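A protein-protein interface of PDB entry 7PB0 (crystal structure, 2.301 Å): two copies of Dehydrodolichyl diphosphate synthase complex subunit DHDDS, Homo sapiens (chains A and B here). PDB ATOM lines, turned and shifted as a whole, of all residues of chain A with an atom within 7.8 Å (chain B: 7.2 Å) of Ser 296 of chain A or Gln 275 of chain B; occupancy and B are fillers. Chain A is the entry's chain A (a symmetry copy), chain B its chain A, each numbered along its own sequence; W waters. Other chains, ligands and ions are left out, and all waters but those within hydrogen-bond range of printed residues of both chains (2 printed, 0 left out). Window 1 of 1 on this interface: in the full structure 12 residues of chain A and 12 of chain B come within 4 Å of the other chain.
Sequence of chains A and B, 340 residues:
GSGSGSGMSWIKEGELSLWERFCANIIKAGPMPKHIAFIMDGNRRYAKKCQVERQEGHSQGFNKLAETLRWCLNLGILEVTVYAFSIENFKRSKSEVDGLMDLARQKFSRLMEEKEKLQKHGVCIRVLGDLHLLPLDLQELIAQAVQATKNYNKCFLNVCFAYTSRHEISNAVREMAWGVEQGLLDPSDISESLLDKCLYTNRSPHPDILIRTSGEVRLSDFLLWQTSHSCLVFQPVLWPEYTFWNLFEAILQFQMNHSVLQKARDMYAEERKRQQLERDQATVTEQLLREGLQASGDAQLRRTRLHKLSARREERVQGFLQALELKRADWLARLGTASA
The side-chain carboxylate (OD1) of Asp 298 of chain A sits close to the side-chain amide oxygen (OE1) of Gln 275 of chain B, 3.0 Å away.
The guanidinium group (NH2) of Arg 274 of chain B lies within salt-bridge range of the side-chain carboxylate (OE2) of Glu 271 of chain B, at 2.4 Å.
The side-chain amide oxygen (OE1) of Gln 275 of chain B sits close to the side-chain carboxylate (OE2) of Glu 271 of chain B (3.2 Å).
NH2 of Arg 272 of chain B lies close to NE2 of Gln 275 of chain B, at 3.3 Å.
NH1 of Arg 274 of chain B is in salt-bridge range of OE2 of Glu 278 of chain B (2.4 Å).
NH2 of Arg 302 of chain A sits at hydrogen-bond distance from O of Ala 295 of chain A (2.5 Å).
Ser 296 of chain A touches Gln 275 of chain B (CB to CG, 3.7 Å).
CB of Ser 296 of chain A touches OE1 of Glu 278 of chain B, 3.4 Å away.
NH2 of Arg 274 of chain B touches O of Gly 297 of chain A, 3.8 Å away.
OE1 of Gln 275 of chain B touches C of Gly 297 of chain A, 3.6 Å away.
OE2 of Glu 271 of chain B touches NE2 of Gln 300 of chain A, at 3.5 Å.
NH2 of Arg 274 of chain B touches CG of Gln 300 of chain A (3.2 Å).
Arg 302 of chain A touches Glu 278 of chain B.
Printed residues of chain B within 4 Å of Asp 298 of chain A: Gln 275 (3.0 Å).
Ala 269 of chain B touches none of the printed residues of chain A.
Of the printed residues of chain A, Arg 274 of chain B touches Gly 297 and Gln 300.
Of chain A, only Ser 296, Gly 297 and Asp 298 come within 4 Å of Gln 275 of chain B.
The nearest residue of chain A that does not touch Gln 275 of chain B is Gln 300 of chain A (5.7 Å).
The nearest printed residue of chain A that does not touch Glu 271 of chain B is Gly 297 of chain A (4.6 Å).
Of the 11 printed residues of chain A, 5 touch a printed residue of chain B.
Printed residues of chain A that touch a printed residue of chain B: Ser 296, Gly 297, Asp 298, Gln 300 and Arg 302.
Of the 14 printed residues of chain B, 4 touch a printed residue of chain A.
Among the printed residues, 8 pairs touch across the chains.
Among the printed residues, no Asp or Glu carboxylate lies within 4 Å of a Lys or Arg side-chain nitrogen of the other chain.
No position is printed for both chains.
Water W1 lies within hydrogen-bond range of the side-chain carboxylate (OE1) of Glu 278 of chain B (3.1 Å), the guanidinium group (NH2) of Arg 274 of chain B (3.2 Å) and the backbone NH (N) of Gly 297 of chain A (3.3 Å).
Water W2 lies within hydrogen-bond range of O of Glu 278 of chain B (3.1 Å) and NH1 of Arg 302 of chain A (3.2 Å).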
ATOM      1  N   LEU A 288      20.542 -12.710 -14.201  1.00  0.00           N
ATOM      2  CA  LEU A 288      20.828 -13.655 -15.273  1.00  0.00           C
ATOM      3  C   LEU A 288      19.705 -13.717 -16.301  1.00  0.00           C
ATOM      4  O   LEU A 288      19.978 -13.881 -17.496  1.00  0.00           O
ATOM      5  CB  LEU A 288      21.095 -15.048 -14.697  1.00  0.00           C
ATOM      6  CG  LEU A 288      22.545 -15.336 -14.321  1.00  0.00           C
ATOM      7  CD1 LEU A 288      22.731 -16.802 -13.983  1.00  0.00           C
ATOM      8  CD2 LEU A 288      23.483 -14.917 -15.441  1.00  0.00           C
ATOM      9  N   LEU A 293      21.469 -15.042 -20.895  1.00  0.00           N
ATOM     10  CA  LEU A 293      21.927 -16.174 -20.084  1.00  0.00           C
ATOM     11  C   LEU A 293      20.897 -16.999 -19.304  1.00  0.00           C
ATOM     12  O   LEU A 293      19.948 -16.485 -18.717  1.00  0.00           O
ATOM     13  CB  LEU A 293      23.034 -15.709 -19.135  1.00  0.00           C
ATOM     14  CG  LEU A 293      23.828 -14.502 -19.632  1.00  0.00           C
ATOM     15  CD1 LEU A 293      24.938 -14.133 -18.661  1.00  0.00           C
ATOM     16  CD2 LEU A 293      24.389 -14.774 -21.018  1.00  0.00           C
ATOM     17  N   GLN A 294      21.136 -18.309 -19.348  1.00  0.00           N
ATOM     18  CA  GLN A 294      20.329 -19.348 -18.735  1.00  0.00           C
ATOM     19  C   GLN A 294      20.424 -19.384 -17.218  1.00  0.00           C
ATOM     20  O   GLN A 294      21.361 -18.868 -16.634  1.00  0.00           O
ATOM     21  CB  GLN A 294      20.755 -20.701 -19.287  1.00  0.00           C
ATOM     22  CG  GLN A 294      20.326 -20.944 -20.715  1.00  0.00           C
ATOM     23  CD  GLN A 294      18.850 -20.731 -20.889  1.00  0.00           C
ATOM     24  OE1 GLN A 294      18.407 -20.203 -21.893  1.00  0.00           O
ATOM     25  NE2 GLN A 294      18.082 -21.132 -19.901  1.00  0.00           N
ATOM     26  N   ALA A 295      19.430 -19.999 -16.593  1.00  0.00           N
ATOM     27  CA  ALA A 295      19.387 -20.164 -15.146  1.00  0.00           C
ATOM     28  C   ALA A 295      20.524 -21.055 -14.650  1.00  0.00           C
ATOM     29  O   ALA A 295      21.079 -20.831 -13.587  1.00  0.00           O
ATOM     30  CB  ALA A 295      18.049 -20.732 -14.719  1.00  0.00           C
ATOM     31  N   SER A 296      20.834 -22.087 -15.425  1.00  0.00           N
ATOM     32  CA  SER A 296      21.889 -23.033 -15.093  1.00  0.00           C
ATOM     33  C   SER A 296      22.655 -23.393 -16.361  1.00  0.00           C
ATOM     34  O   SER A 296      22.188 -23.173 -17.481  1.00  0.00           O
ATOM     35  CB  SER A 296      21.329 -24.299 -14.427  1.00  0.00           C
ATOM     36  N   GLY A 297      23.844 -23.943 -16.175  1.00  0.00           N
ATOM     37  CA  GLY A 297      24.639 -24.368 -17.312  1.00  0.00           C
ATOM     38  C   GLY A 297      25.958 -24.934 -16.838  1.00  0.00           C
ATOM     39  O   GLY A 297      26.355 -24.762 -15.680  1.00  0.00           O
ATOM     40  N   ASP A 298      26.634 -25.622 -17.760  1.00  0.00           N
ATOM     41  CA  ASP A 298      27.924 -26.212 -17.430  1.00  0.00           C
ATOM     42  C   ASP A 298      28.954 -25.140 -17.116  1.00  0.00           C
ATOM     43  O   ASP A 298      29.878 -25.379 -16.329  1.00  0.00           O
ATOM     44  CB  ASP A 298      28.412 -27.096 -18.574  1.00  0.00           C
ATOM     45  CG  ASP A 298      27.587 -28.352 -18.726  1.00  0.00           C
ATOM     46  OD1 ASP A 298      26.566 -28.474 -18.015  1.00  0.00           O
ATOM     47  OD2 ASP A 298      27.947 -29.213 -19.559  1.00  0.00           O
ATOM     48  N   ALA A 299      28.810 -23.956 -17.716  1.00  0.00           N
ATOM     49  CA  ALA A 299      29.723 -22.862 -17.422  1.00  0.00           C
ATOM     50  C   ALA A 299      29.666 -22.461 -15.958  1.00  0.00           C
ATOM     51  O   ALA A 299      30.616 -21.852 -15.458  1.00  0.00           O
ATOM     52  CB  ALA A 299      29.413 -21.661 -18.315  1.00  0.00           C
ATOM     53  N   GLN A 300      28.580 -22.807 -15.264  1.00  0.00           N
ATOM     54  CA  GLN A 300      28.422 -22.553 -13.835  1.00  0.00           C
ATOM     55  C   GLN A 300      28.631 -21.077 -13.518  1.00  0.00           C
ATOM     56  O   GLN A 300      29.333 -20.709 -12.576  1.00  0.00           O
ATOM     57  CB  GLN A 300      29.366 -23.431 -13.014  1.00  0.00           C
ATOM     58  CG  GLN A 300      28.816 -24.812 -12.730  1.00  0.00           C
ATOM     59  CD  GLN A 300      29.900 -25.816 -12.421  1.00  0.00           C
ATOM     60  OE1 GLN A 300      30.824 -25.534 -11.658  1.00  0.00           O
ATOM     61  NE2 GLN A 300      29.795 -27.000 -13.014  1.00  0.00           N
ATOM     62  N   LEU A 301      28.018 -20.222 -14.335  1.00  0.00           N
ATOM     63  CA  LEU A 301      28.172 -18.791 -14.120  1.00  0.00           C
ATOM     64  C   LEU A 301      27.308 -18.294 -12.969  1.00  0.00           C
ATOM     65  O   LEU A 301      27.658 -17.298 -12.326  1.00  0.00           O
ATOM     66  CB  LEU A 301      27.883 -18.019 -15.414  1.00  0.00           C
ATOM     67  CG  LEU A 301      26.508 -17.940 -16.073  1.00  0.00           C
ATOM     68  CD1 LEU A 301      26.546 -16.855 -17.144  1.00  0.00           C
ATOM     69  CD2 LEU A 301      26.092 -19.274 -16.687  1.00  0.00           C
ATOM     70  N   ARG A 302      26.196 -18.975 -12.681  1.00  0.00           N
ATOM     71  CA  ARG A 302      25.468 -18.690 -11.450  1.00  0.00           C
ATOM     72  C   ARG A 302      26.384 -18.827 -10.243  1.00  0.00           C
ATOM     73  O   ARG A 302      26.350 -18.001  -9.322  1.00  0.00           O
ATOM     74  CB  ARG A 302      24.265 -19.628 -11.317  1.00  0.00           C
ATOM     75  CG  ARG A 302      24.037 -20.155  -9.900  1.00  0.00           C
ATOM     76  CD  ARG A 302      22.627 -20.702  -9.715  1.00  0.00           C
ATOM     77  NE  ARG A 302      21.652 -19.630  -9.558  1.00  0.00           N
ATOM     78  CZ  ARG A 302      20.563 -19.510 -10.304  1.00  0.00           C
ATOM     79  NH1 ARG A 302      19.732 -18.501 -10.103  1.00  0.00           N
ATOM     80  NH2 ARG A 302      20.308 -20.401 -11.253  1.00  0.00           N
ATOM     81  N   ALA B 269      25.592 -37.305 -13.313  1.00  0.00           N
ATOM     82  CA  ALA B 269      24.281 -37.396 -12.679  1.00  0.00           C
ATOM     83  C   ALA B 269      24.104 -36.326 -11.611  1.00  0.00           C
ATOM     84  O   ALA B 269      23.055 -35.673 -11.542  1.00  0.00           O
ATOM     85  CB  ALA B 269      24.089 -38.786 -12.078  1.00  0.00           C
ATOM     86  N   GLU B 270      25.114 -36.133 -10.765  1.00  0.00           N
ATOM     87  CA  GLU B 270      25.004 -35.125  -9.720  1.00  0.00           C
ATOM     88  C   GLU B 270      24.922 -33.726 -10.313  1.00  0.00           C
ATOM     89  O   GLU B 270      24.250 -32.850  -9.756  1.00  0.00           O
ATOM     90  CB  GLU B 270      26.187 -35.238  -8.755  1.00  0.00           C
ATOM     91  N   GLU B 271      25.581 -33.503 -11.452  1.00  0.00           N
ATOM     92  CA  GLU B 271      25.530 -32.187 -12.079  1.00  0.00           C
ATOM     93  C   GLU B 271      24.173 -31.935 -12.722  1.00  0.00           C
ATOM     94  O   GLU B 271      23.670 -30.805 -12.698  1.00  0.00           O
ATOM     95  CB  GLU B 271      26.652 -32.054 -13.108  1.00  0.00           C
ATOM     96  CG  GLU B 271      26.800 -30.658 -13.698  1.00  0.00           C
ATOM     97  CD  GLU B 271      27.011 -29.581 -12.645  1.00  0.00           C
ATOM     98  OE1 GLU B 271      27.593 -29.882 -11.579  1.00  0.00           O
ATOM     99  OE2 GLU B 271      26.590 -28.429 -12.889  1.00  0.00           O
ATOM    100  N   ARG B 272      23.564 -32.973 -13.296  1.00  0.00           N
ATOM    101  CA  ARG B 272      22.233 -32.817 -13.871  1.00  0.00           C
ATOM    102  C   ARG B 272      21.201 -32.499 -12.796  1.00  0.00           C
ATOM    103  O   ARG B 272      20.378 -31.594 -12.971  1.00  0.00           O
ATOM    104  CB  ARG B 272      21.839 -34.076 -14.640  1.00  0.00           C
ATOM    105  CG  ARG B 272      22.687 -34.344 -15.882  1.00  0.00           C
ATOM    106  CD  ARG B 272      22.964 -33.078 -16.691  1.00  0.00           C
ATOM    107  NE  ARG B 272      21.740 -32.415 -17.137  1.00  0.00           N
ATOM    108  CZ  ARG B 272      21.711 -31.235 -17.751  1.00  0.00           C
ATOM    109  NH1 ARG B 272      20.555 -30.699 -18.120  1.00  0.00           N
ATOM    110  NH2 ARG B 272      22.839 -30.586 -17.996  1.00  0.00           N
ATOM    111  N   LYS B 273      21.233 -33.222 -11.672  1.00  0.00           N
ATOM    112  CA  LYS B 273      20.271 -32.952 -10.604  1.00  0.00           C
ATOM    113  C   LYS B 273      20.486 -31.566 -10.011  1.00  0.00           C
ATOM    114  O   LYS B 273      19.520 -30.872  -9.674  1.00  0.00           O
ATOM    115  CB  LYS B 273      20.361 -34.027  -9.517  1.00  0.00           C
ATOM    116  N   ARG B 274      21.744 -31.138  -9.893  1.00  0.00           N
ATOM    117  CA  ARG B 274      22.028 -29.789  -9.411  1.00  0.00           C
ATOM    118  C   ARG B 274      21.410 -28.737 -10.327  1.00  0.00           C
ATOM    119  O   ARG B 274      20.734 -27.813  -9.864  1.00  0.00           O
ATOM    120  CB  ARG B 274      23.540 -29.587  -9.291  1.00  0.00           C
ATOM    121  CG  ARG B 274      23.957 -28.193  -8.844  1.00  0.00           C
ATOM    122  CD  ARG B 274      25.454 -27.978  -9.012  1.00  0.00           C
ATOM    123  NE  ARG B 274      25.814 -27.631 -10.386  1.00  0.00           N
ATOM    124  CZ  ARG B 274      25.644 -26.426 -10.925  1.00  0.00           C
ATOM    125  NH1 ARG B 274      25.121 -25.443 -10.209  1.00  0.00           N
ATOM    126  NH2 ARG B 274      25.996 -26.202 -12.183  1.00  0.00           N
ATOM    127  N   GLN B 275      21.621 -28.872 -11.639  1.00  0.00           N
ATOM    128  CA  GLN B 275      21.095 -27.890 -12.582  1.00  0.00           C
ATOM    129  C   GLN B 275      19.570 -27.904 -12.613  1.00  0.00           C
ATOM    130  O   GLN B 275      18.935 -26.850 -12.740  1.00  0.00           O
ATOM    131  CB  GLN B 275      21.682 -28.140 -13.976  1.00  0.00           C
ATOM    132  CG  GLN B 275      23.077 -27.527 -14.143  1.00  0.00           C
ATOM    133  CD  GLN B 275      23.715 -27.783 -15.504  1.00  0.00           C
ATOM    134  OE1 GLN B 275      24.889 -28.150 -15.585  1.00  0.00           O
ATOM    135  NE2 GLN B 275      22.955 -27.570 -16.573  1.00  0.00           N
ATOM    136  N   GLN B 276      18.961 -29.083 -12.482  1.00  0.00           N
ATOM    137  CA  GLN B 276      17.505 -29.159 -12.447  1.00  0.00           C
ATOM    138  C   GLN B 276      16.950 -28.441 -11.223  1.00  0.00           C
ATOM    139  O   GLN B 276      15.949 -27.719 -11.317  1.00  0.00           O
ATOM    140  CB  GLN B 276      17.053 -30.618 -12.460  1.00  0.00           C
ATOM    141  CG  GLN B 276      15.546 -30.804 -12.473  1.00  0.00           C
ATOM    142  CD  GLN B 276      14.941 -30.519 -13.832  1.00  0.00           C
ATOM    143  OE1 GLN B 276      15.177 -31.251 -14.796  1.00  0.00           O
ATOM    144  NE2 GLN B 276      14.153 -29.450 -13.918  1.00  0.00           N
ATOM    145  N   LEU B 277      17.591 -28.632 -10.065  1.00  0.00           N
ATOM    146  CA  LEU B 277      17.173 -27.934  -8.853  1.00  0.00           C
ATOM    147  C   LEU B 277      17.295 -26.424  -9.016  1.00  0.00           C
ATOM    148  O   LEU B 277      16.427 -25.669  -8.561  1.00  0.00           O
ATOM    149  CB  LEU B 277      18.004 -28.414  -7.661  1.00  0.00           C
ATOM    150  CG  LEU B 277      17.732 -27.754  -6.308  1.00  0.00           C
ATOM    151  CD1 LEU B 277      16.299 -27.994  -5.865  1.00  0.00           C
ATOM    152  CD2 LEU B 277      18.700 -28.275  -5.263  1.00  0.00           C
ATOM    153  N   GLU B 278      18.363 -25.965  -9.670  1.00  0.00           N
ATOM    154  CA  GLU B 278      18.518 -24.531  -9.894  1.00  0.00           C
ATOM    155  C   GLU B 278      17.443 -24.005 -10.834  1.00  0.00           C
ATOM    156  O   GLU B 278      16.907 -22.911 -10.621  1.00  0.00           O
ATOM    157  CB  GLU B 278      19.913 -24.231 -10.442  1.00  0.00           C
ATOM    158  CG  GLU B 278      21.005 -24.284  -9.386  1.00  0.00           C
ATOM    159  CD  GLU B 278      22.403 -24.183  -9.967  1.00  0.00           C
ATOM    160  OE1 GLU B 278      22.545 -24.204 -11.212  1.00  0.00           O
ATOM    161  OE2 GLU B 278      23.368 -24.097  -9.172  1.00  0.00           O
ATOM    162  N   ARG B 279      17.114 -24.769 -11.878  1.00  0.00           N
ATOM    163  CA  ARG B 279      16.075 -24.343 -12.810  1.00  0.00           C
ATOM    164  C   ARG B 279      14.717 -24.289 -12.124  1.00  0.00           C
ATOM    165  O   ARG B 279      13.969 -23.315 -12.277  1.00  0.00           O
ATOM    166  CB  ARG B 279      16.033 -25.285 -14.017  1.00  0.00           C
ATOM    167  CG  ARG B 279      16.845 -24.818 -15.214  1.00  0.00           C
ATOM    168  CD  ARG B 279      17.087 -25.956 -16.193  1.00  0.00           C
ATOM    169  N   ASP B 280      14.392 -25.324 -11.348  1.00  0.00           N
ATOM    170  CA  ASP B 280      13.111 -25.353 -10.650  1.00  0.00           C
ATOM    171  C   ASP B 280      13.001 -24.212  -9.646  1.00  0.00           C
ATOM    172  O   ASP B 280      11.950 -23.569  -9.539  1.00  0.00           O
ATOM    173  CB  ASP B 280      12.924 -26.699  -9.954  1.00  0.00           C
ATOM    174  CG  ASP B 280      12.665 -27.827 -10.932  1.00  0.00           C
ATOM    175  OD1 ASP B 280      12.105 -27.555 -12.018  1.00  0.00           O
ATOM    176  OD2 ASP B 280      13.015 -28.984 -10.609  1.00  0.00           O
ATOM    177  N   GLN B 281      14.074 -23.932  -8.906  1.00  0.00           N
ATOM    178  CA  GLN B 281      13.970 -22.872  -7.916  1.00  0.00           C
ATOM    179  C   GLN B 281      13.969 -21.488  -8.550  1.00  0.00           C
ATOM    180  O   GLN B 281      13.420 -20.552  -7.956  1.00  0.00           O
ATOM    181  CB  GLN B 281      15.077 -23.009  -6.879  1.00  0.00           C
ATOM    182  CG  GLN B 281      14.527 -23.589  -5.589  1.00  0.00           C
ATOM    183  CD  GLN B 281      15.579 -23.835  -4.544  1.00  0.00           C
ATOM    184  OE1 GLN B 281      16.702 -24.227  -4.857  1.00  0.00           O
ATOM    185  NE2 GLN B 281      15.218 -23.619  -3.286  1.00  0.00           N
ATOM    186  N   ALA B 282      14.536 -21.341  -9.750  1.00  0.00           N
ATOM    187  CA  ALA B 282      14.356 -20.095 -10.489  1.00  0.00           C
ATOM    188  C   ALA B 282      12.912 -19.946 -10.955  1.00  0.00           C
ATOM    189  O   ALA B 282      12.366 -18.838 -10.950  1.00  0.00           O
ATOM    190  CB  ALA B 282      15.320 -20.036 -11.672  1.00  0.00           C
HETATM  191  O   HOH W   1      24.817 -23.363 -13.099  1.00  0.00           O
HETATM  192  O   HOH W   2      18.210 -20.880  -8.691  1.00  0.00           O
